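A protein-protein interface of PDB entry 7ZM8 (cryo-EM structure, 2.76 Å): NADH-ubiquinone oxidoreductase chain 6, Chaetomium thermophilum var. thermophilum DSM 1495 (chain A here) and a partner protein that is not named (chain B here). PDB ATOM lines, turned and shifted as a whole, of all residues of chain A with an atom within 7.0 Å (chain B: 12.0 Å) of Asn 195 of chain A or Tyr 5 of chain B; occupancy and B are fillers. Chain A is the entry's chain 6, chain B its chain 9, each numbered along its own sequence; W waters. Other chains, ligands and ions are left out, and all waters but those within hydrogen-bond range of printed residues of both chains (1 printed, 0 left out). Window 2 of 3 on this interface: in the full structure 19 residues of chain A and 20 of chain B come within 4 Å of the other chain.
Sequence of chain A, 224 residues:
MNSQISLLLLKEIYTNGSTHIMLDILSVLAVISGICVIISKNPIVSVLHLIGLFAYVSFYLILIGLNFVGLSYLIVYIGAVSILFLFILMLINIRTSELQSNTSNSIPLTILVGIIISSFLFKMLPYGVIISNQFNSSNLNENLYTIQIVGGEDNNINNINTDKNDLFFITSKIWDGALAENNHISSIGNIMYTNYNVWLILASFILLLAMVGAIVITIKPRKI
No residue of chain B comes within 4 Å of Thr 194 of chain A.
Asn 195 of chain A touches one residue of chain B.
Tyr 196 of chain A touches just these residues of chain B: Ser 3 (3.9 Å) and Tyr 5 (3.9 Å).
No residue of chain B comes within 4 Å of Asn 197 of chain A.
Of the printed residues of chain A, Ser 3 of chain B touches Tyr 196 (3.9 Å).
No residue of chain A comes within 4 Å of Gly 4 of chain B.
Of chain A, only Ile 191, Asn 195 and Tyr 196 come within 4 Å of Tyr 5 of chain B.
Printed residues of chain A within 4 Å of Asn 8 of chain B: Ser 187 (3.9 Å).
Ser 12 of chain B touches none of the printed residues of chain A.
Trp 18 of chain B touches none of the printed residues of chain A.
Of the 10 printed residues of chain A, 4 touch a printed residue of chain B.
Hydrophobic or aromatic side chains of chain A that line the printed part of chain B: Ile 191 and Tyr 196.
Among the printed residues, no Asp or Glu carboxylate lies within 4 Å of a Lys or Arg side-chain nitrogen of the other chain.
O of Leu 7 of chain B lies within hydrogen-bond range of OG of Ser 187 of chain A (3.2 Å).
The side-chain hydroxyl of Ser 187 of chain A sits at hydrogen-bond distance from the backbone NH of Gly 9 of chain B, at 3.3 Å.
The side-chain hydroxyl of Tyr 5 of chain B sits at hydrogen-bond distance from the side-chain amide oxygen of Asn 195 of chain A (2.9 Å).
Water W1 lies within hydrogen-bond range of the side-chain hydroxyl of Tyr 5 of chain B (3.1 Å), the side-chain amide oxygen of Asn 195 of chain A (3.1 Å) and the side-chain hydroxyl of Tyr 196 of chain A (3.3 Å).
OG1 of Thr 194 of chain A lies within hydrogen-bond range of ND2 of Asn 195 of chain A (3.1 Å).
The backbone NH of Tyr 5 of chain B sits at hydrogen-bond distance from the side-chain hydroxyl of Ser 3 of chain B (3.1 Å).
The backbone carbonyl oxygen (O) of Ile 191 of chain A is in hydrogen-bond range of the backbone NH (N) of Tyr 196 of chain A (3.3 Å).
Among the printed residues, merely in contact across the chains: Ile 191 of chain A with Tyr 5 of chain B, Tyr 196 of chain A with Tyr 5 of chain B, Tyr 196 of chain A with Ser 3 of chain B and Ser 187 of chain A with Asn 8 of chain B.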
ATOM      1  N   SER A 187      21.400  31.555  -8.939  1.00  0.00           N
ATOM      2  CA  SER A 187      20.823  30.327  -8.347  1.00  0.00           C
ATOM      3  C   SER A 187      21.553  29.059  -8.822  1.00  0.00           C
ATOM      4  O   SER A 187      21.765  28.175  -7.985  1.00  0.00           O
ATOM      5  CB  SER A 187      19.362  30.303  -8.652  1.00  0.00           C
ATOM      6  OG  SER A 187      18.802  31.592  -8.510  1.00  0.00           O
ATOM      7  N   ASN A 190      24.846  29.106  -7.053  1.00  0.00           N
ATOM      8  CA  ASN A 190      24.744  28.775  -5.616  1.00  0.00           C
ATOM      9  C   ASN A 190      24.895  27.269  -5.420  1.00  0.00           C
ATOM     10  O   ASN A 190      25.436  26.883  -4.389  1.00  0.00           O
ATOM     11  CB  ASN A 190      23.425  29.240  -5.004  1.00  0.00           C
ATOM     12  CG  ASN A 190      23.266  30.737  -4.870  1.00  0.00           C
ATOM     13  OD1 ASN A 190      24.210  31.496  -5.052  1.00  0.00           O
ATOM     14  ND2 ASN A 190      22.059  31.168  -4.551  1.00  0.00           N
ATOM     15  N   ILE A 191      24.456  26.442  -6.363  1.00  0.00           N
ATOM     16  CA  ILE A 191      24.478  24.967  -6.129  1.00  0.00           C
ATOM     17  C   ILE A 191      25.474  24.256  -7.053  1.00  0.00           C
ATOM     18  O   ILE A 191      25.834  23.115  -6.731  1.00  0.00           O
ATOM     19  CB  ILE A 191      23.039  24.415  -6.277  1.00  0.00           C
ATOM     20  CG1 ILE A 191      22.528  24.545  -7.713  1.00  0.00           C
ATOM     21  CG2 ILE A 191      22.099  25.070  -5.284  1.00  0.00           C
ATOM     22  CD1 ILE A 191      21.550  23.476  -8.114  1.00  0.00           C
ATOM     23  N   MET A 192      25.936  24.909  -8.122  1.00  0.00           N
ATOM     24  CA  MET A 192      26.744  24.264  -9.149  1.00  0.00           C
ATOM     25  C   MET A 192      28.124  23.871  -8.636  1.00  0.00           C
ATOM     26  O   MET A 192      28.725  22.916  -9.139  1.00  0.00           O
ATOM     27  CB  MET A 192      26.855  25.207 -10.342  1.00  0.00           C
ATOM     28  CG  MET A 192      27.854  24.851 -11.399  1.00  0.00           C
ATOM     29  SD  MET A 192      27.716  25.992 -12.775  1.00  0.00           S
ATOM     30  CE  MET A 192      28.948  25.296 -13.854  1.00  0.00           C
ATOM     31  N   TYR A 193      28.661  24.620  -7.670  1.00  0.00           N
ATOM     32  CA  TYR A 193      30.056  24.391  -7.239  1.00  0.00           C
ATOM     33  C   TYR A 193      30.138  23.799  -5.839  1.00  0.00           C
ATOM     34  O   TYR A 193      31.241  23.620  -5.346  1.00  0.00           O
ATOM     35  CB  TYR A 193      30.849  25.692  -7.329  1.00  0.00           C
ATOM     36  CG  TYR A 193      30.721  26.433  -8.626  1.00  0.00           C
ATOM     37  CD1 TYR A 193      31.563  26.160  -9.686  1.00  0.00           C
ATOM     38  CD2 TYR A 193      29.758  27.409  -8.781  1.00  0.00           C
ATOM     39  CE1 TYR A 193      31.444  26.839 -10.883  1.00  0.00           C
ATOM     40  CE2 TYR A 193      29.615  28.088  -9.972  1.00  0.00           C
ATOM     41  CZ  TYR A 193      30.468  27.807 -11.020  1.00  0.00           C
ATOM     42  OH  TYR A 193      30.340  28.502 -12.178  1.00  0.00           O
ATOM     43  N   THR A 194      28.994  23.470  -5.239  1.00  0.00           N
ATOM     44  CA  THR A 194      28.980  22.936  -3.852  1.00  0.00           C
ATOM     45  C   THR A 194      28.194  21.629  -3.788  1.00  0.00           C
ATOM     46  O   THR A 194      28.834  20.577  -3.774  1.00  0.00           O
ATOM     47  CB  THR A 194      28.466  23.990  -2.862  1.00  0.00           C
ATOM     48  OG1 THR A 194      27.286  24.579  -3.407  1.00  0.00           O
ATOM     49  CG2 THR A 194      29.482  25.071  -2.569  1.00  0.00           C
ATOM     50  N   ASN A 195      26.864  21.700  -3.771  1.00  0.00           N
ATOM     51  CA  ASN A 195      25.989  20.508  -3.602  1.00  0.00           C
ATOM     52  C   ASN A 195      26.138  19.493  -4.736  1.00  0.00           C
ATOM     53  O   ASN A 195      26.179  18.293  -4.434  1.00  0.00           O
ATOM     54  CB  ASN A 195      24.522  20.937  -3.535  1.00  0.00           C
ATOM     55  CG  ASN A 195      24.182  21.895  -2.415  1.00  0.00           C
ATOM     56  OD1 ASN A 195      23.427  21.547  -1.513  1.00  0.00           O
ATOM     57  ND2 ASN A 195      24.700  23.110  -2.476  1.00  0.00           N
ATOM     58  N   TYR A 196      26.228  19.951  -5.981  1.00  0.00           N
ATOM     59  CA  TYR A 196      26.264  19.041  -7.156  1.00  0.00           C
ATOM     60  C   TYR A 196      27.630  19.167  -7.833  1.00  0.00           C
ATOM     61  O   TYR A 196      27.684  19.027  -9.064  1.00  0.00           O
ATOM     62  CB  TYR A 196      25.078  19.317  -8.081  1.00  0.00           C
ATOM     63  CG  TYR A 196      23.723  19.184  -7.435  1.00  0.00           C
ATOM     64  CD1 TYR A 196      23.082  20.279  -6.883  1.00  0.00           C
ATOM     65  CD2 TYR A 196      23.084  17.960  -7.368  1.00  0.00           C
ATOM     66  CE1 TYR A 196      21.841  20.163  -6.282  1.00  0.00           C
ATOM     67  CE2 TYR A 196      21.842  17.825  -6.772  1.00  0.00           C
ATOM     68  CZ  TYR A 196      21.218  18.930  -6.227  1.00  0.00           C
ATOM     69  OH  TYR A 196      19.994  18.802  -5.640  1.00  0.00           O
ATOM     70  N   ASN A 197      28.695  19.396  -7.059  1.00  0.00           N
ATOM     71  CA  ASN A 197      30.058  19.630  -7.617  1.00  0.00           C
ATOM     72  C   ASN A 197      30.616  18.409  -8.360  1.00  0.00           C
ATOM     73  O   ASN A 197      31.547  18.595  -9.148  1.00  0.00           O
ATOM     74  CB  ASN A 197      31.006  20.258  -6.586  1.00  0.00           C
ATOM     75  CG  ASN A 197      31.326  19.383  -5.395  1.00  0.00           C
ATOM     76  OD1 ASN A 197      30.858  18.253  -5.293  1.00  0.00           O
ATOM     77  ND2 ASN A 197      32.130  19.903  -4.483  1.00  0.00           N
ATOM     78  N   VAL A 198      30.115  17.210  -8.075  1.00  0.00           N
ATOM     79  CA  VAL A 198      30.580  15.959  -8.753  1.00  0.00           C
ATOM     80  C   VAL A 198      30.276  16.043 -10.254  1.00  0.00           C
ATOM     81  O   VAL A 198      31.099  15.557 -11.043  1.00  0.00           O
ATOM     82  CB  VAL A 198      30.020  14.691  -8.069  1.00  0.00           C
ATOM     83  CG1 VAL A 198      29.630  13.592  -9.047  1.00  0.00           C
ATOM     84  CG2 VAL A 198      30.980  14.163  -7.019  1.00  0.00           C
ATOM     85  N   ALA B   2      11.630  18.414  -6.637  1.00  0.00           N
ATOM     86  CA  ALA B   2      12.117  17.436  -5.627  1.00  0.00           C
ATOM     87  C   ALA B   2      13.568  17.722  -5.227  1.00  0.00           C
ATOM     88  O   ALA B   2      14.047  17.066  -4.299  1.00  0.00           O
ATOM     89  CB  ALA B   2      11.993  16.025  -6.144  1.00  0.00           C
ATOM     90  N   SER B   3      14.215  18.711  -5.842  1.00  0.00           N
ATOM     91  CA  SER B   3      15.645  18.997  -5.560  1.00  0.00           C
ATOM     92  C   SER B   3      15.686  19.892  -4.331  1.00  0.00           C
ATOM     93  O   SER B   3      16.558  19.690  -3.479  1.00  0.00           O
ATOM     94  CB  SER B   3      16.344  19.638  -6.706  1.00  0.00           C
ATOM     95  OG  SER B   3      16.067  21.023  -6.771  1.00  0.00           O
ATOM     96  N   GLY B   4      14.720  20.786  -4.225  1.00  0.00           N
ATOM     97  CA  GLY B   4      14.691  21.724  -3.125  1.00  0.00           C
ATOM     98  C   GLY B   4      15.262  23.082  -3.442  1.00  0.00           C
ATOM     99  O   GLY B   4      15.329  23.928  -2.547  1.00  0.00           O
ATOM    100  N   TYR B   5      15.693  23.318  -4.675  1.00  0.00           N
ATOM    101  CA  TYR B   5      16.221  24.604  -5.102  1.00  0.00           C
ATOM    102  C   TYR B   5      15.389  25.098  -6.272  1.00  0.00           C
ATOM    103  O   TYR B   5      15.194  24.373  -7.251  1.00  0.00           O
ATOM    104  CB  TYR B   5      17.705  24.485  -5.468  1.00  0.00           C
ATOM    105  CG  TYR B   5      18.498  23.818  -4.374  1.00  0.00           C
ATOM    106  CD1 TYR B   5      18.641  22.441  -4.339  1.00  0.00           C
ATOM    107  CD2 TYR B   5      19.064  24.559  -3.347  1.00  0.00           C
ATOM    108  CE1 TYR B   5      19.332  21.826  -3.330  1.00  0.00           C
ATOM    109  CE2 TYR B   5      19.770  23.950  -2.335  1.00  0.00           C
ATOM    110  CZ  TYR B   5      19.896  22.580  -2.329  1.00  0.00           C
ATOM    111  OH  TYR B   5      20.590  21.956  -1.323  1.00  0.00           O
ATOM    112  N   GLY B   6      14.861  26.310  -6.153  1.00  0.00           N
ATOM    113  CA  GLY B   6      14.004  26.887  -7.197  1.00  0.00           C
ATOM    114  C   GLY B   6      14.703  27.918  -8.043  1.00  0.00           C
ATOM    115  O   GLY B   6      15.883  28.175  -7.804  1.00  0.00           O
ATOM    116  N   LEU B   7      13.976  28.511  -8.978  1.00  0.00           N
ATOM    117  CA  LEU B   7      14.556  29.471  -9.943  1.00  0.00           C
ATOM    118  C   LEU B   7      14.989  30.799  -9.318  1.00  0.00           C
ATOM    119  O   LEU B   7      15.893  31.416  -9.888  1.00  0.00           O
ATOM    120  CB  LEU B   7      13.530  29.662 -11.065  1.00  0.00           C
ATOM    121  CG  LEU B   7      12.880  28.387 -11.599  1.00  0.00           C
ATOM    122  CD1 LEU B   7      11.792  28.723 -12.602  1.00  0.00           C
ATOM    123  CD2 LEU B   7      13.911  27.478 -12.236  1.00  0.00           C
ATOM    124  N   ASN B   8      14.410  31.217  -8.191  1.00  0.00           N
ATOM    125  CA  ASN B   8      14.643  32.577  -7.635  1.00  0.00           C
ATOM    126  C   ASN B   8      15.605  32.616  -6.452  1.00  0.00           C
ATOM    127  O   ASN B   8      15.602  33.625  -5.736  1.00  0.00           O
ATOM    128  CB  ASN B   8      13.335  33.185  -7.139  1.00  0.00           C
ATOM    129  CG  ASN B   8      12.814  32.491  -5.898  1.00  0.00           C
ATOM    130  OD1 ASN B   8      12.628  31.277  -5.889  1.00  0.00           O
ATOM    131  ND2 ASN B   8      12.598  33.254  -4.842  1.00  0.00           N
ATOM    132  N   GLY B   9      16.424  31.604  -6.248  1.00  0.00           N
ATOM    133  CA  GLY B   9      17.220  31.603  -5.010  1.00  0.00           C
ATOM    134  C   GLY B   9      16.679  30.569  -4.055  1.00  0.00           C
ATOM    135  O   GLY B   9      17.185  30.512  -2.941  1.00  0.00           O
ATOM    136  N   GLY B  10      15.628  29.845  -4.445  1.00  0.00           N
ATOM    137  CA  GLY B  10      15.175  28.675  -3.677  1.00  0.00           C
ATOM    138  C   GLY B  10      14.074  28.962  -2.707  1.00  0.00           C
ATOM    139  O   GLY B  10      13.913  30.167  -2.477  1.00  0.00           O
ATOM    140  N   PRO B  11      13.382  27.964  -2.068  1.00  0.00           N
ATOM    141  CA  PRO B  11      13.349  26.558  -2.488  1.00  0.00           C
ATOM    142  C   PRO B  11      12.359  26.286  -3.612  1.00  0.00           C
ATOM    143  O   PRO B  11      11.744  27.226  -4.109  1.00  0.00           O
ATOM    144  CB  PRO B  11      12.922  25.826  -1.215  1.00  0.00           C
ATOM    145  CG  PRO B  11      13.052  26.835  -0.115  1.00  0.00           C
ATOM    146  CD  PRO B  11      12.753  28.132  -0.753  1.00  0.00           C
ATOM    147  N   SER B  12      12.209  24.993  -3.943  1.00  0.00           N
ATOM    148  CA  SER B  12      11.299  24.565  -5.040  1.00  0.00           C
ATOM    149  C   SER B  12       9.863  24.392  -4.542  1.00  0.00           C
ATOM    150  O   SER B  12       9.699  23.937  -3.426  1.00  0.00           O
ATOM    151  CB  SER B  12      11.831  23.371  -5.795  1.00  0.00           C
ATOM    152  OG  SER B  12      12.192  22.313  -4.935  1.00  0.00           O
ATOM    153  N   ARG B  13       8.864  24.685  -5.371  1.00  0.00           N
ATOM    154  CA  ARG B  13       7.436  24.689  -4.935  1.00  0.00           C
ATOM    155  C   ARG B  13       6.933  23.329  -4.465  1.00  0.00           C
ATOM    156  O   ARG B  13       6.109  23.315  -3.550  1.00  0.00           O
ATOM    157  CB  ARG B  13       6.518  25.274  -6.015  1.00  0.00           C
ATOM    158  CG  ARG B  13       6.651  24.647  -7.390  1.00  0.00           C
ATOM    159  CD  ARG B  13       5.624  25.263  -8.313  1.00  0.00           C
ATOM    160  NE  ARG B  13       5.511  24.434  -9.495  1.00  0.00           N
ATOM    161  CZ  ARG B  13       4.654  23.436  -9.606  1.00  0.00           C
ATOM    162  NH1 ARG B  13       4.621  22.711 -10.708  1.00  0.00           N
ATOM    163  NH2 ARG B  13       3.834  23.169  -8.610  1.00  0.00           N
ATOM    164  N   CYS B  14       7.360  22.250  -5.101  1.00  0.00           N
ATOM    165  CA  CYS B  14       6.813  20.922  -4.762  1.00  0.00           C
ATOM    166  C   CYS B  14       7.687  20.217  -3.736  1.00  0.00           C
ATOM    167  O   CYS B  14       7.346  19.101  -3.383  1.00  0.00           O
ATOM    168  CB  CYS B  14       6.622  20.126  -6.040  1.00  0.00           C
ATOM    169  SG  CYS B  14       5.294  20.822  -7.054  1.00  0.00           S
ATOM    170  N   PHE B  15       8.794  20.810  -3.322  1.00  0.00           N
ATOM    171  CA  PHE B  15       9.704  20.172  -2.337  1.00  0.00           C
ATOM    172  C   PHE B  15       8.974  19.809  -1.033  1.00  0.00           C
ATOM    173  O   PHE B  15       9.272  18.739  -0.502  1.00  0.00           O
ATOM    174  CB  PHE B  15      10.975  20.999  -2.162  1.00  0.00           C
ATOM    175  CG  PHE B  15      12.038  20.367  -1.305  1.00  0.00           C
ATOM    176  CD1 PHE B  15      12.702  19.229  -1.730  1.00  0.00           C
ATOM    177  CD2 PHE B  15      12.389  20.920  -0.087  1.00  0.00           C
ATOM    178  CE1 PHE B  15      13.692  18.658  -0.952  1.00  0.00           C
ATOM    179  CE2 PHE B  15      13.379  20.345   0.690  1.00  0.00           C
ATOM    180  CZ  PHE B  15      14.032  19.219   0.252  1.00  0.00           C
ATOM    181  N   PRO B  16       8.027  20.600  -0.479  1.00  0.00           N
ATOM    182  CA  PRO B  16       7.341  20.181   0.740  1.00  0.00           C
ATOM    183  C   PRO B  16       6.595  18.842   0.613  1.00  0.00           C
ATOM    184  O   PRO B  16       6.735  18.040   1.491  1.00  0.00           O
ATOM    185  CB  PRO B  16       6.349  21.323   0.956  1.00  0.00           C
ATOM    186  CG  PRO B  16       7.042  22.515   0.402  1.00  0.00           C
ATOM    187  CD  PRO B  16       7.675  21.971  -0.854  1.00  0.00           C
ATOM    188  N   PHE B  17       5.904  18.607  -0.495  1.00  0.00           N
ATOM    189  CA  PHE B  17       5.180  17.343  -0.765  1.00  0.00           C
ATOM    190  C   PHE B  17       6.137  16.157  -0.865  1.00  0.00           C
ATOM    191  O   PHE B  17       5.750  15.086  -0.412  1.00  0.00           O
ATOM    192  CB  PHE B  17       4.358  17.532  -2.044  1.00  0.00           C
ATOM    193  CG  PHE B  17       3.236  18.533  -1.936  1.00  0.00           C
ATOM    194  CD1 PHE B  17       3.459  19.882  -2.164  1.00  0.00           C
ATOM    195  CD2 PHE B  17       1.960  18.125  -1.591  1.00  0.00           C
ATOM    196  CE1 PHE B  17       2.425  20.798  -2.059  1.00  0.00           C
ATOM    197  CE2 PHE B  17       0.929  19.044  -1.483  1.00  0.00           C
ATOM    198  CZ  PHE B  17       1.162  20.376  -1.723  1.00  0.00           C
ATOM    199  N   TRP B  18       7.290  16.328  -1.498  1.00  0.00           N
ATOM    200  CA  TRP B  18       8.320  15.268  -1.649  1.00  0.00           C
ATOM    201  C   TRP B  18       8.878  14.848  -0.290  1.00  0.00           C
ATOM    202  O   TRP B  18       9.063  13.662  -0.089  1.00  0.00           O
ATOM    203  CB  TRP B  18       9.439  15.811  -2.549  1.00  0.00           C
ATOM    204  CG  TRP B  18      10.541  14.836  -2.815  1.00  0.00           C
ATOM    205  CD1 TRP B  18      11.830  14.906  -2.376  1.00  0.00           C
ATOM    206  CD2 TRP B  18      10.442  13.626  -3.581  1.00  0.00           C
ATOM    207  NE1 TRP B  18      12.542  13.828  -2.824  1.00  0.00           N
ATOM    208  CE2 TRP B  18      11.719  13.029  -3.571  1.00  0.00           C
ATOM    209  CE3 TRP B  18       9.406  12.992  -4.270  1.00  0.00           C
ATOM    210  CZ2 TRP B  18      11.977  11.823  -4.220  1.00  0.00           C
ATOM    211  CZ3 TRP B  18       9.664  11.807  -4.917  1.00  0.00           C
ATOM    212  CH2 TRP B  18      10.934  11.235  -4.894  1.00  0.00           C
ATOM    213  N   GLN B  19       9.160  15.811   0.584  1.00  0.00           N
ATOM    214  CA  GLN B  19       9.678  15.517   1.940  1.00  0.00           C
ATOM    215  C   GLN B  19       8.560  14.866   2.749  1.00  0.00           C
ATOM    216  O   GLN B  19       8.875  14.002   3.563  1.00  0.00           O
ATOM    217  CB  GLN B  19      10.148  16.813   2.586  1.00  0.00           C
ATOM    218  CG  GLN B  19      11.372  17.402   1.912  1.00  0.00           C
ATOM    219  CD  GLN B  19      12.496  17.607   2.894  1.00  0.00           C
ATOM    220  OE1 GLN B  19      13.522  16.938   2.839  1.00  0.00           O
ATOM    221  NE2 GLN B  19      12.303  18.542   3.808  1.00  0.00           N
ATOM    222  N   TYR B  47       1.834  14.781  -4.499  1.00  0.00           N
ATOM    223  CA  TYR B  47       3.113  15.235  -5.068  1.00  0.00           C
ATOM    224  C   TYR B  47       3.035  15.168  -6.594  1.00  0.00           C
ATOM    225  O   TYR B  47       3.539  16.084  -7.236  1.00  0.00           O
ATOM    226  CB  TYR B  47       4.241  14.357  -4.530  1.00  0.00           C
ATOM    227  CG  TYR B  47       5.548  14.565  -5.247  1.00  0.00           C
ATOM    228  CD1 TYR B  47       6.277  15.725  -5.063  1.00  0.00           C
ATOM    229  CD2 TYR B  47       6.022  13.629  -6.149  1.00  0.00           C
ATOM    230  CE1 TYR B  47       7.462  15.942  -5.739  1.00  0.00           C
ATOM    231  CE2 TYR B  47       7.204  13.832  -6.834  1.00  0.00           C
ATOM    232  CZ  TYR B  47       7.925  14.990  -6.624  1.00  0.00           C
ATOM    233  OH  TYR B  47       9.096  15.193  -7.285  1.00  0.00           O
ATOM    234  N   LEU B  51       3.282  18.699  -9.028  1.00  0.00           N
ATOM    235  CA  LEU B  51       4.077  18.862 -10.265  1.00  0.00           C
ATOM    236  C   LEU B  51       3.213  19.096 -11.497  1.00  0.00           C
ATOM    237  O   LEU B  51       3.565  19.999 -12.264  1.00  0.00           O
ATOM    238  CB  LEU B  51       4.889  17.594 -10.528  1.00  0.00           C
ATOM    239  CG  LEU B  51       5.847  17.094  -9.455  1.00  0.00           C
ATOM    240  CD1 LEU B  51       6.240  15.665  -9.778  1.00  0.00           C
ATOM    241  CD2 LEU B  51       7.085  17.971  -9.380  1.00  0.00           C
HETATM  242  O   HOH W   1      21.494  19.412  -2.782  1.00  0.00           O
